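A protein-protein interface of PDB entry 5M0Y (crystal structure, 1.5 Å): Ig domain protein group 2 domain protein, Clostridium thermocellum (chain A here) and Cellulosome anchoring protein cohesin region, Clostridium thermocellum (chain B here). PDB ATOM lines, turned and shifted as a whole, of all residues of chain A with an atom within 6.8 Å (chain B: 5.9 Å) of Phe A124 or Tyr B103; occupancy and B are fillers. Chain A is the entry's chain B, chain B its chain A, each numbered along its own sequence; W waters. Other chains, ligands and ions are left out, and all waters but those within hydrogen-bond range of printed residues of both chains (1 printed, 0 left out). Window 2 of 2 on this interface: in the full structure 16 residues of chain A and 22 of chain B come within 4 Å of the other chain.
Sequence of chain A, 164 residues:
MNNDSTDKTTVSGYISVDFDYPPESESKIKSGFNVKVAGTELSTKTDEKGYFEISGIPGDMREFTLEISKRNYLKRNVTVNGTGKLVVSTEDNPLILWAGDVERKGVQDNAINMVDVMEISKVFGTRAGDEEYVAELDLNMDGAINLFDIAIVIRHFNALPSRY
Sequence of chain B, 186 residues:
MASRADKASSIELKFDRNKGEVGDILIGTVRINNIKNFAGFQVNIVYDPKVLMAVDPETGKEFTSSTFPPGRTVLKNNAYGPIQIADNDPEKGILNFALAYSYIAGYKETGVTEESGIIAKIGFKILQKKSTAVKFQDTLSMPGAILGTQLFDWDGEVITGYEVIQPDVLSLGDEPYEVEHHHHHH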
ATOM      1  N   GLU A 119      -5.294  -7.321 -11.184  1.00  0.00           N
ATOM      2  CA  GLU A 119      -6.588  -6.959 -11.763  1.00  0.00           C
ATOM      3  C   GLU A 119      -6.395  -6.448 -13.195  1.00  0.00           C
ATOM      4  O   GLU A 119      -7.155  -6.819 -14.104  1.00  0.00           O
ATOM      5  CB  GLU A 119      -7.291  -5.919 -10.888  1.00  0.00           C
ATOM      6  CG  GLU A 119      -8.669  -5.485 -11.361  1.00  0.00           C
ATOM      7  CD  GLU A 119      -9.706  -6.580 -11.421  1.00  0.00           C
ATOM      8  OE1 GLU A 119      -9.536  -7.645 -10.795  1.00  0.00           O
ATOM      9  OE2 GLU A 119     -10.732  -6.343 -12.103  1.00  0.00           O
ATOM     10  N   ILE A 120      -5.377  -5.617 -13.398  1.00  0.00           N
ATOM     11  CA  ILE A 120      -5.035  -5.133 -14.743  1.00  0.00           C
ATOM     12  C   ILE A 120      -4.586  -6.303 -15.617  1.00  0.00           C
ATOM     13  O   ILE A 120      -4.949  -6.384 -16.796  1.00  0.00           O
ATOM     14  CB  ILE A 120      -3.966  -4.021 -14.693  1.00  0.00           C
ATOM     15  CG1 ILE A 120      -4.540  -2.789 -13.985  1.00  0.00           C
ATOM     16  CG2 ILE A 120      -3.500  -3.631 -16.094  1.00  0.00           C
ATOM     17  CD1 ILE A 120      -3.502  -1.781 -13.578  1.00  0.00           C
ATOM     18  N   SER A 121      -3.827  -7.222 -15.030  1.00  0.00           N
ATOM     19  CA  SER A 121      -3.318  -8.364 -15.779  1.00  0.00           C
ATOM     20  C   SER A 121      -4.422  -9.241 -16.382  1.00  0.00           C
ATOM     21  O   SER A 121      -4.206  -9.871 -17.411  1.00  0.00           O
ATOM     22  CB  SER A 121      -2.365  -9.179 -14.907  1.00  0.00           C
ATOM     23  OG  SER A 121      -1.219  -8.401 -14.599  1.00  0.00           O
ATOM     24  N   LYS A 122      -5.603  -9.259 -15.762  1.00  0.00           N
ATOM     25  CA  LYS A 122      -6.767 -10.014 -16.287  1.00  0.00           C
ATOM     26  C   LYS A 122      -7.102  -9.660 -17.732  1.00  0.00           C
ATOM     27  O   LYS A 122      -7.573 -10.523 -18.481  1.00  0.00           O
ATOM     28  CB  LYS A 122      -8.024  -9.781 -15.446  1.00  0.00           C
ATOM     29  CG  LYS A 122      -8.008 -10.365 -14.047  1.00  0.00           C
ATOM     30  CD  LYS A 122      -9.301 -10.024 -13.326  1.00  0.00           C
ATOM     31  CE  LYS A 122      -9.330 -10.598 -11.925  1.00  0.00           C
ATOM     32  NZ  LYS A 122     -10.579 -10.228 -11.210  1.00  0.00           N
ATOM     33  N   VAL A 123      -6.866  -8.401 -18.099  1.00  0.00           N
ATOM     34  CA  VAL A 123      -7.166  -7.896 -19.444  1.00  0.00           C
ATOM     35  C   VAL A 123      -5.912  -7.396 -20.169  1.00  0.00           C
ATOM     36  O   VAL A 123      -5.981  -6.518 -21.033  1.00  0.00           O
ATOM     37  CB  VAL A 123      -8.274  -6.821 -19.385  1.00  0.00           C
ATOM     38  CG1 VAL A 123      -9.579  -7.462 -18.936  1.00  0.00           C
ATOM     39  CG2 VAL A 123      -7.902  -5.681 -18.455  1.00  0.00           C
ATOM     40  N   PHE A 124      -4.769  -8.003 -19.853  1.00  0.00           N
ATOM     41  CA  PHE A 124      -3.501  -7.630 -20.440  1.00  0.00           C
ATOM     42  C   PHE A 124      -3.499  -7.894 -21.941  1.00  0.00           C
ATOM     43  O   PHE A 124      -3.984  -8.934 -22.397  1.00  0.00           O
ATOM     44  CB  PHE A 124      -2.375  -8.438 -19.799  1.00  0.00           C
ATOM     45  CG  PHE A 124      -1.010  -8.038 -20.256  1.00  0.00           C
ATOM     46  CD1 PHE A 124      -0.344  -6.987 -19.640  1.00  0.00           C
ATOM     47  CD2 PHE A 124      -0.383  -8.718 -21.297  1.00  0.00           C
ATOM     48  CE1 PHE A 124       0.926  -6.614 -20.053  1.00  0.00           C
ATOM     49  CE2 PHE A 124       0.887  -8.348 -21.717  1.00  0.00           C
ATOM     50  CZ  PHE A 124       1.544  -7.298 -21.089  1.00  0.00           C
ATOM     51  N   GLY A 125      -2.965  -6.936 -22.692  1.00  0.00           N
ATOM     52  CA  GLY A 125      -2.882  -7.042 -24.148  1.00  0.00           C
ATOM     53  C   GLY A 125      -4.151  -6.723 -24.917  1.00  0.00           C
ATOM     54  O   GLY A 125      -4.178  -6.904 -26.143  1.00  0.00           O
ATOM     55  N   THR A 126      -5.206  -6.260 -24.236  1.00  0.00           N
ATOM     56  CA  THR A 126      -6.447  -5.883 -24.919  1.00  0.00           C
ATOM     57  C   THR A 126      -6.312  -4.469 -25.465  1.00  0.00           C
ATOM     58  O   THR A 126      -5.496  -3.681 -24.981  1.00  0.00           O
ATOM     59  CB  THR A 126      -7.687  -5.971 -24.008  1.00  0.00           C
ATOM     60  OG1 THR A 126      -7.492  -5.147 -22.854  1.00  0.00           O
ATOM     61  CG2 THR A 126      -7.950  -7.415 -23.569  1.00  0.00           C
ATOM     62  N   ILE A 145      -4.324  -1.899 -23.014  1.00  0.00           N
ATOM     63  CA  ILE A 145      -3.975  -2.277 -21.645  1.00  0.00           C
ATOM     64  C   ILE A 145      -2.731  -3.146 -21.713  1.00  0.00           C
ATOM     65  O   ILE A 145      -2.765  -4.254 -22.258  1.00  0.00           O
ATOM     66  CB  ILE A 145      -5.124  -3.000 -20.924  1.00  0.00           C
ATOM     67  CG1 ILE A 145      -6.323  -2.053 -20.822  1.00  0.00           C
ATOM     68  CG2 ILE A 145      -4.673  -3.437 -19.530  1.00  0.00           C
ATOM     69  CD1 ILE A 145      -7.595  -2.685 -20.317  1.00  0.00           C
ATOM     70  N   ASN A 146      -1.633  -2.635 -21.166  1.00  0.00           N
ATOM     71  CA  ASN A 146      -0.336  -3.260 -21.353  1.00  0.00           C
ATOM     72  C   ASN A 146       0.653  -2.851 -20.251  1.00  0.00           C
ATOM     73  O   ASN A 146       0.228  -2.384 -19.193  1.00  0.00           O
ATOM     74  CB  ASN A 146       0.149  -2.973 -22.787  1.00  0.00           C
ATOM     75  CG  ASN A 146       0.427  -1.501 -23.055  1.00  0.00           C
ATOM     76  OD1 ASN A 146       0.688  -0.715 -22.149  1.00  0.00           O
ATOM     77  ND2 ASN A 146       0.398  -1.128 -24.335  1.00  0.00           N
ATOM     78  N   LEU A 147       1.949  -3.049 -20.468  1.00  0.00           N
ATOM     79  CA  LEU A 147       2.930  -2.835 -19.411  1.00  0.00           C
ATOM     80  C   LEU A 147       3.071  -1.382 -18.956  1.00  0.00           C
ATOM     81  O   LEU A 147       3.481  -1.150 -17.825  1.00  0.00           O
ATOM     82  CB  LEU A 147       4.295  -3.414 -19.806  1.00  0.00           C
ATOM     83  CG  LEU A 147       4.323  -4.941 -19.935  1.00  0.00           C
ATOM     84  CD1 LEU A 147       5.602  -5.374 -20.641  1.00  0.00           C
ATOM     85  CD2 LEU A 147       4.165  -5.628 -18.590  1.00  0.00           C
ATOM     86  N   PHE A 148       2.724  -0.410 -19.807  1.00  0.00           N
ATOM     87  CA  PHE A 148       2.710   0.995 -19.369  1.00  0.00           C
ATOM     88  C   PHE A 148       1.696   1.226 -18.249  1.00  0.00           C
ATOM     89  O   PHE A 148       1.977   1.970 -17.313  1.00  0.00           O
ATOM     90  CB  PHE A 148       2.400   1.953 -20.521  1.00  0.00           C
ATOM     91  CG  PHE A 148       3.503   2.089 -21.540  1.00  0.00           C
ATOM     92  CD1 PHE A 148       4.832   2.257 -21.157  1.00  0.00           C
ATOM     93  CD2 PHE A 148       3.195   2.114 -22.899  1.00  0.00           C
ATOM     94  CE1 PHE A 148       5.835   2.410 -22.107  1.00  0.00           C
ATOM     95  CE2 PHE A 148       4.194   2.268 -23.853  1.00  0.00           C
ATOM     96  CZ  PHE A 148       5.514   2.415 -23.454  1.00  0.00           C
ATOM     97  N   ILE A 150       0.553  -1.166 -16.144  1.00  0.00           N
ATOM     98  CA  ILE A 150       1.110  -1.860 -14.984  1.00  0.00           C
ATOM     99  C   ILE A 150       2.241  -1.043 -14.339  1.00  0.00           C
ATOM    100  O   ILE A 150       2.317  -0.950 -13.112  1.00  0.00           O
ATOM    101  CB  ILE A 150       1.536  -3.305 -15.343  1.00  0.00           C
ATOM    102  CG1 ILE A 150       0.272  -4.151 -15.552  1.00  0.00           C
ATOM    103  CG2 ILE A 150       2.417  -3.913 -14.253  1.00  0.00           C
ATOM    104  CD1 ILE A 150       0.507  -5.505 -16.174  1.00  0.00           C
ATOM    105  N   ALA B  79       7.247 -16.068 -22.280  1.00  0.00           N
ATOM    106  CA  ALA B  79       6.019 -16.091 -23.084  1.00  0.00           C
ATOM    107  C   ALA B  79       4.827 -15.441 -22.380  1.00  0.00           C
ATOM    108  O   ALA B  79       3.928 -14.928 -23.047  1.00  0.00           O
ATOM    109  CB  ALA B  79       5.659 -17.515 -23.485  1.00  0.00           C
ATOM    110  N   TYR B  80       4.818 -15.467 -21.043  1.00  0.00           N
ATOM    111  CA  TYR B  80       3.718 -14.888 -20.259  1.00  0.00           C
ATOM    112  C   TYR B  80       4.069 -13.577 -19.550  1.00  0.00           C
ATOM    113  O   TYR B  80       3.322 -13.132 -18.677  1.00  0.00           O
ATOM    114  CB  TYR B  80       3.199 -15.917 -19.250  1.00  0.00           C
ATOM    115  CG  TYR B  80       3.048 -17.304 -19.837  1.00  0.00           C
ATOM    116  CD1 TYR B  80       2.252 -17.515 -20.961  1.00  0.00           C
ATOM    117  CD2 TYR B  80       3.720 -18.395 -19.291  1.00  0.00           C
ATOM    118  CE1 TYR B  80       2.125 -18.782 -21.511  1.00  0.00           C
ATOM    119  CE2 TYR B  80       3.594 -19.662 -19.833  1.00  0.00           C
ATOM    120  CZ  TYR B  80       2.797 -19.842 -20.948  1.00  0.00           C
ATOM    121  OH  TYR B  80       2.665 -21.092 -21.496  1.00  0.00           O
ATOM    122  N   GLY B  81       5.177 -12.944 -19.932  1.00  0.00           N
ATOM    123  CA  GLY B  81       5.531 -11.624 -19.413  1.00  0.00           C
ATOM    124  C   GLY B  81       5.715 -11.507 -17.905  1.00  0.00           C
ATOM    125  O   GLY B  81       5.022 -10.724 -17.264  1.00  0.00           O
ATOM    126  N   ILE B  83       6.881 -10.187 -14.450  1.00  0.00           N
ATOM    127  CA  ILE B  83       7.206  -8.836 -13.981  1.00  0.00           C
ATOM    128  C   ILE B  83       7.674  -8.904 -12.531  1.00  0.00           C
ATOM    129  O   ILE B  83       6.943  -9.407 -11.683  1.00  0.00           O
ATOM    130  CB  ILE B  83       5.973  -7.916 -14.005  1.00  0.00           C
ATOM    131  CG1 ILE B  83       5.384  -7.812 -15.404  1.00  0.00           C
ATOM    132  CG2 ILE B  83       6.333  -6.514 -13.526  1.00  0.00           C
ATOM    133  CD1 ILE B  83       4.413  -6.664 -15.503  1.00  0.00           C
ATOM    134  N   TYR B 101       3.217 -13.487 -13.641  1.00  0.00           N
ATOM    135  CA  TYR B 101       2.992 -13.373 -15.073  1.00  0.00           C
ATOM    136  C   TYR B 101       1.962 -12.276 -15.321  1.00  0.00           C
ATOM    137  O   TYR B 101       0.860 -12.325 -14.775  1.00  0.00           O
ATOM    138  CB  TYR B 101       2.497 -14.695 -15.643  1.00  0.00           C
ATOM    139  CG  TYR B 101       3.521 -15.810 -15.725  1.00  0.00           C
ATOM    140  CD1 TYR B 101       4.859 -15.558 -16.073  1.00  0.00           C
ATOM    141  CD2 TYR B 101       3.144 -17.132 -15.524  1.00  0.00           C
ATOM    142  CE1 TYR B 101       5.779 -16.590 -16.184  1.00  0.00           C
ATOM    143  CE2 TYR B 101       4.058 -18.169 -15.644  1.00  0.00           C
ATOM    144  CZ  TYR B 101       5.375 -17.895 -15.975  1.00  0.00           C
ATOM    145  OH  TYR B 101       6.284 -18.926 -16.090  1.00  0.00           O
ATOM    146  N   SER B 102       2.317 -11.287 -16.138  1.00  0.00           N
ATOM    147  CA  SER B 102       1.365 -10.250 -16.538  1.00  0.00           C
ATOM    148  C   SER B 102       0.352 -10.773 -17.550  1.00  0.00           C
ATOM    149  O   SER B 102      -0.807 -10.368 -17.537  1.00  0.00           O
ATOM    150  CB  SER B 102       2.086  -9.011 -17.072  1.00  0.00           C
ATOM    151  OG  SER B 102       2.889  -9.292 -18.198  1.00  0.00           O
ATOM    152  N   TYR B 103       0.778 -11.693 -18.416  1.00  0.00           N
ATOM    153  CA  TYR B 103      -0.128 -12.255 -19.411  1.00  0.00           C
ATOM    154  C   TYR B 103      -0.688 -13.592 -18.926  1.00  0.00           C
ATOM    155  O   TYR B 103      -0.377 -14.664 -19.447  1.00  0.00           O
ATOM    156  CB  TYR B 103       0.573 -12.368 -20.767  1.00  0.00           C
ATOM    157  CG  TYR B 103      -0.345 -12.784 -21.891  1.00  0.00           C
ATOM    158  CD1 TYR B 103      -1.606 -12.205 -22.039  1.00  0.00           C
ATOM    159  CD2 TYR B 103       0.044 -13.753 -22.810  1.00  0.00           C
ATOM    160  CE1 TYR B 103      -2.456 -12.584 -23.059  1.00  0.00           C
ATOM    161  CE2 TYR B 103      -0.805 -14.139 -23.837  1.00  0.00           C
ATOM    162  CZ  TYR B 103      -2.047 -13.548 -23.955  1.00  0.00           C
ATOM    163  OH  TYR B 103      -2.888 -13.928 -24.968  1.00  0.00           O
ATOM    164  N   ILE B 104      -1.526 -13.503 -17.896  1.00  0.00           N
ATOM    165  CA  ILE B 104      -2.127 -14.695 -17.294  1.00  0.00           C
ATOM    166  C   ILE B 104      -3.065 -15.466 -18.220  1.00  0.00           C
ATOM    167  O   ILE B 104      -3.149 -16.692 -18.124  1.00  0.00           O
ATOM    168  CB  ILE B 104      -2.844 -14.406 -15.951  1.00  0.00           C
ATOM    169  CG1 ILE B 104      -3.774 -13.182 -16.033  1.00  0.00           C
ATOM    170  CG2 ILE B 104      -1.822 -14.218 -14.841  1.00  0.00           C
ATOM    171  CD1 ILE B 104      -4.668 -13.024 -14.824  1.00  0.00           C
ATOM    172  N   ALA B 105      -3.744 -14.767 -19.126  1.00  0.00           N
ATOM    173  CA  ALA B 105      -4.609 -15.434 -20.099  1.00  0.00           C
ATOM    174  C   ALA B 105      -3.827 -16.410 -20.992  1.00  0.00           C
ATOM    175  O   ALA B 105      -4.311 -17.502 -21.281  1.00  0.00           O
ATOM    176  CB  ALA B 105      -5.360 -14.415 -20.945  1.00  0.00           C
ATOM    177  N   GLY B 106      -2.622 -16.025 -21.410  1.00  0.00           N
ATOM    178  CA  GLY B 106      -1.759 -16.936 -22.178  1.00  0.00           C
ATOM    179  C   GLY B 106      -1.310 -18.146 -21.387  1.00  0.00           C
ATOM    180  O   GLY B 106      -1.314 -19.280 -21.880  1.00  0.00           O
ATOM    181  N   TYR B 107      -0.897 -17.891 -20.147  1.00  0.00           N
ATOM    182  CA  TYR B 107      -0.511 -18.935 -19.214  1.00  0.00           C
ATOM    183  C   TYR B 107      -1.647 -19.943 -19.012  1.00  0.00           C
ATOM    184  O   TYR B 107      -1.446 -21.155 -19.132  1.00  0.00           O
ATOM    185  CB  TYR B 107      -0.062 -18.264 -17.908  1.00  0.00           C
ATOM    186  CG  TYR B 107       0.250 -19.167 -16.750  1.00  0.00           C
ATOM    187  CD1 TYR B 107       1.071 -20.287 -16.887  1.00  0.00           C
ATOM    188  CD2 TYR B 107      -0.238 -18.868 -15.481  1.00  0.00           C
ATOM    189  CE1 TYR B 107       1.355 -21.099 -15.800  1.00  0.00           C
ATOM    190  CE2 TYR B 107       0.042 -19.671 -14.394  1.00  0.00           C
ATOM    191  CZ  TYR B 107       0.835 -20.789 -14.553  1.00  0.00           C
ATOM    192  OH  TYR B 107       1.120 -21.579 -13.469  1.00  0.00           O
ATOM    193  N   LYS B 108      -2.844 -19.436 -18.754  1.00  0.00           N
ATOM    194  CA  LYS B 108      -4.021 -20.284 -18.608  1.00  0.00           C
ATOM    195  C   LYS B 108      -4.342 -21.077 -19.874  1.00  0.00           C
ATOM    196  O   LYS B 108      -4.654 -22.262 -19.793  1.00  0.00           O
ATOM    197  CB  LYS B 108      -5.229 -19.449 -18.180  1.00  0.00           C
ATOM    198  CG  LYS B 108      -6.477 -20.279 -17.936  1.00  0.00           C
ATOM    199  CD  LYS B 108      -7.578 -19.476 -17.274  1.00  0.00           C
ATOM    200  CE  LYS B 108      -8.726 -20.412 -16.943  1.00  0.00           C
ATOM    201  NZ  LYS B 108      -9.895 -19.726 -16.341  1.00  0.00           N
ATOM    202  N   GLU B 109      -4.261 -20.424 -21.028  1.00  0.00           N
ATOM    203  CA  GLU B 109      -4.591 -21.088 -22.291  1.00  0.00           C
ATOM    204  C   GLU B 109      -3.679 -22.272 -22.583  1.00  0.00           C
ATOM    205  O   GLU B 109      -4.154 -23.321 -23.015  1.00  0.00           O
ATOM    206  CB  GLU B 109      -4.548 -20.102 -23.448  1.00  0.00           C
ATOM    207  CG  GLU B 109      -5.042 -20.718 -24.747  1.00  0.00           C
ATOM    208  CD  GLU B 109      -5.332 -19.689 -25.811  1.00  0.00           C
ATOM    209  OE1 GLU B 109      -4.763 -18.584 -25.758  1.00  0.00           O
ATOM    210  OE2 GLU B 109      -6.151 -19.989 -26.700  1.00  0.00           O
HETATM  211  O   HOH W   1      -3.856 -11.864 -19.340  1.00  0.00           O
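O of Ser B102 lies close to O of Ser A121 (3.4 Å).
The side-chain carboxylate (OE1) of Glu A119 lies within salt-bridge range of the side-chain amino group (NZ) of Lys A122 (2.8 Å).
The backbone carbonyl oxygen (O) of Tyr B80 lies within hydrogen-bond range of the backbone NH (N) of Ser B102.
The backbone carbonyl oxygen (O) of Tyr B80 sits at hydrogen-bond distance from the backbone NH (N) of Tyr B103.
The backbone carbonyl oxygen (O) of Gly B81 lies within hydrogen-bond range of the side-chain hydroxyl (OG) of Ser B102, 2.7 Å away.
Among the printed residues, pairs that only touch across the chains: Leu A147 with Ile B83 (3.3 Å), Phe A124 with Ser B102 (3.4 Å), Ser A121 with Ile B104 (3.6 Å), Ile A150 with Ile B83 (3.6 Å), Phe A124 with Tyr B103 (3.8 Å), Leu A147 with Ser B102 (3.9 Å), Ile A150 with Ser B102 (3.9 Å) and Lys A122 with Ile B104 (3.95 Å).
Of chain A, only Phe A124 (3.8 Å) comes within 4 Å of Tyr B103.
Printed residues of chain B within 4 Å of Leu A147: Ile B83 and Ser B102.
Printed residues of chain A within 4 Å of Ile B104: Ser A121 and Lys A122.
Printed residues of chain A within 4 Å of Ile B83: Leu A147 (3.3 Å) and Ile A150 (3.6 Å).
The nearest printed residue of chain A that does not touch Tyr B103 is Ser A121 (5.1 Å).
Hydrophobic or aromatic side chains of chain A that line the printed part of chain B: Phe A124, Leu A147 and Ile A150.
Of the 13 printed residues of chain B, 4 touch a printed residue of chain A.
Hydrophobic or aromatic side chains of chain B that line the printed part of chain A: Ile B83, Tyr B103 and Ile B104.
Among the printed residues, 9 pairs touch across the chains.
Water W1 lies within hydrogen-bond range of the backbone carbonyl oxygen of Ser A121 (2.8 Å), the backbone NH of Ala B105 (2.9 Å) and the backbone NH of Ile B104 (3.2 Å).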
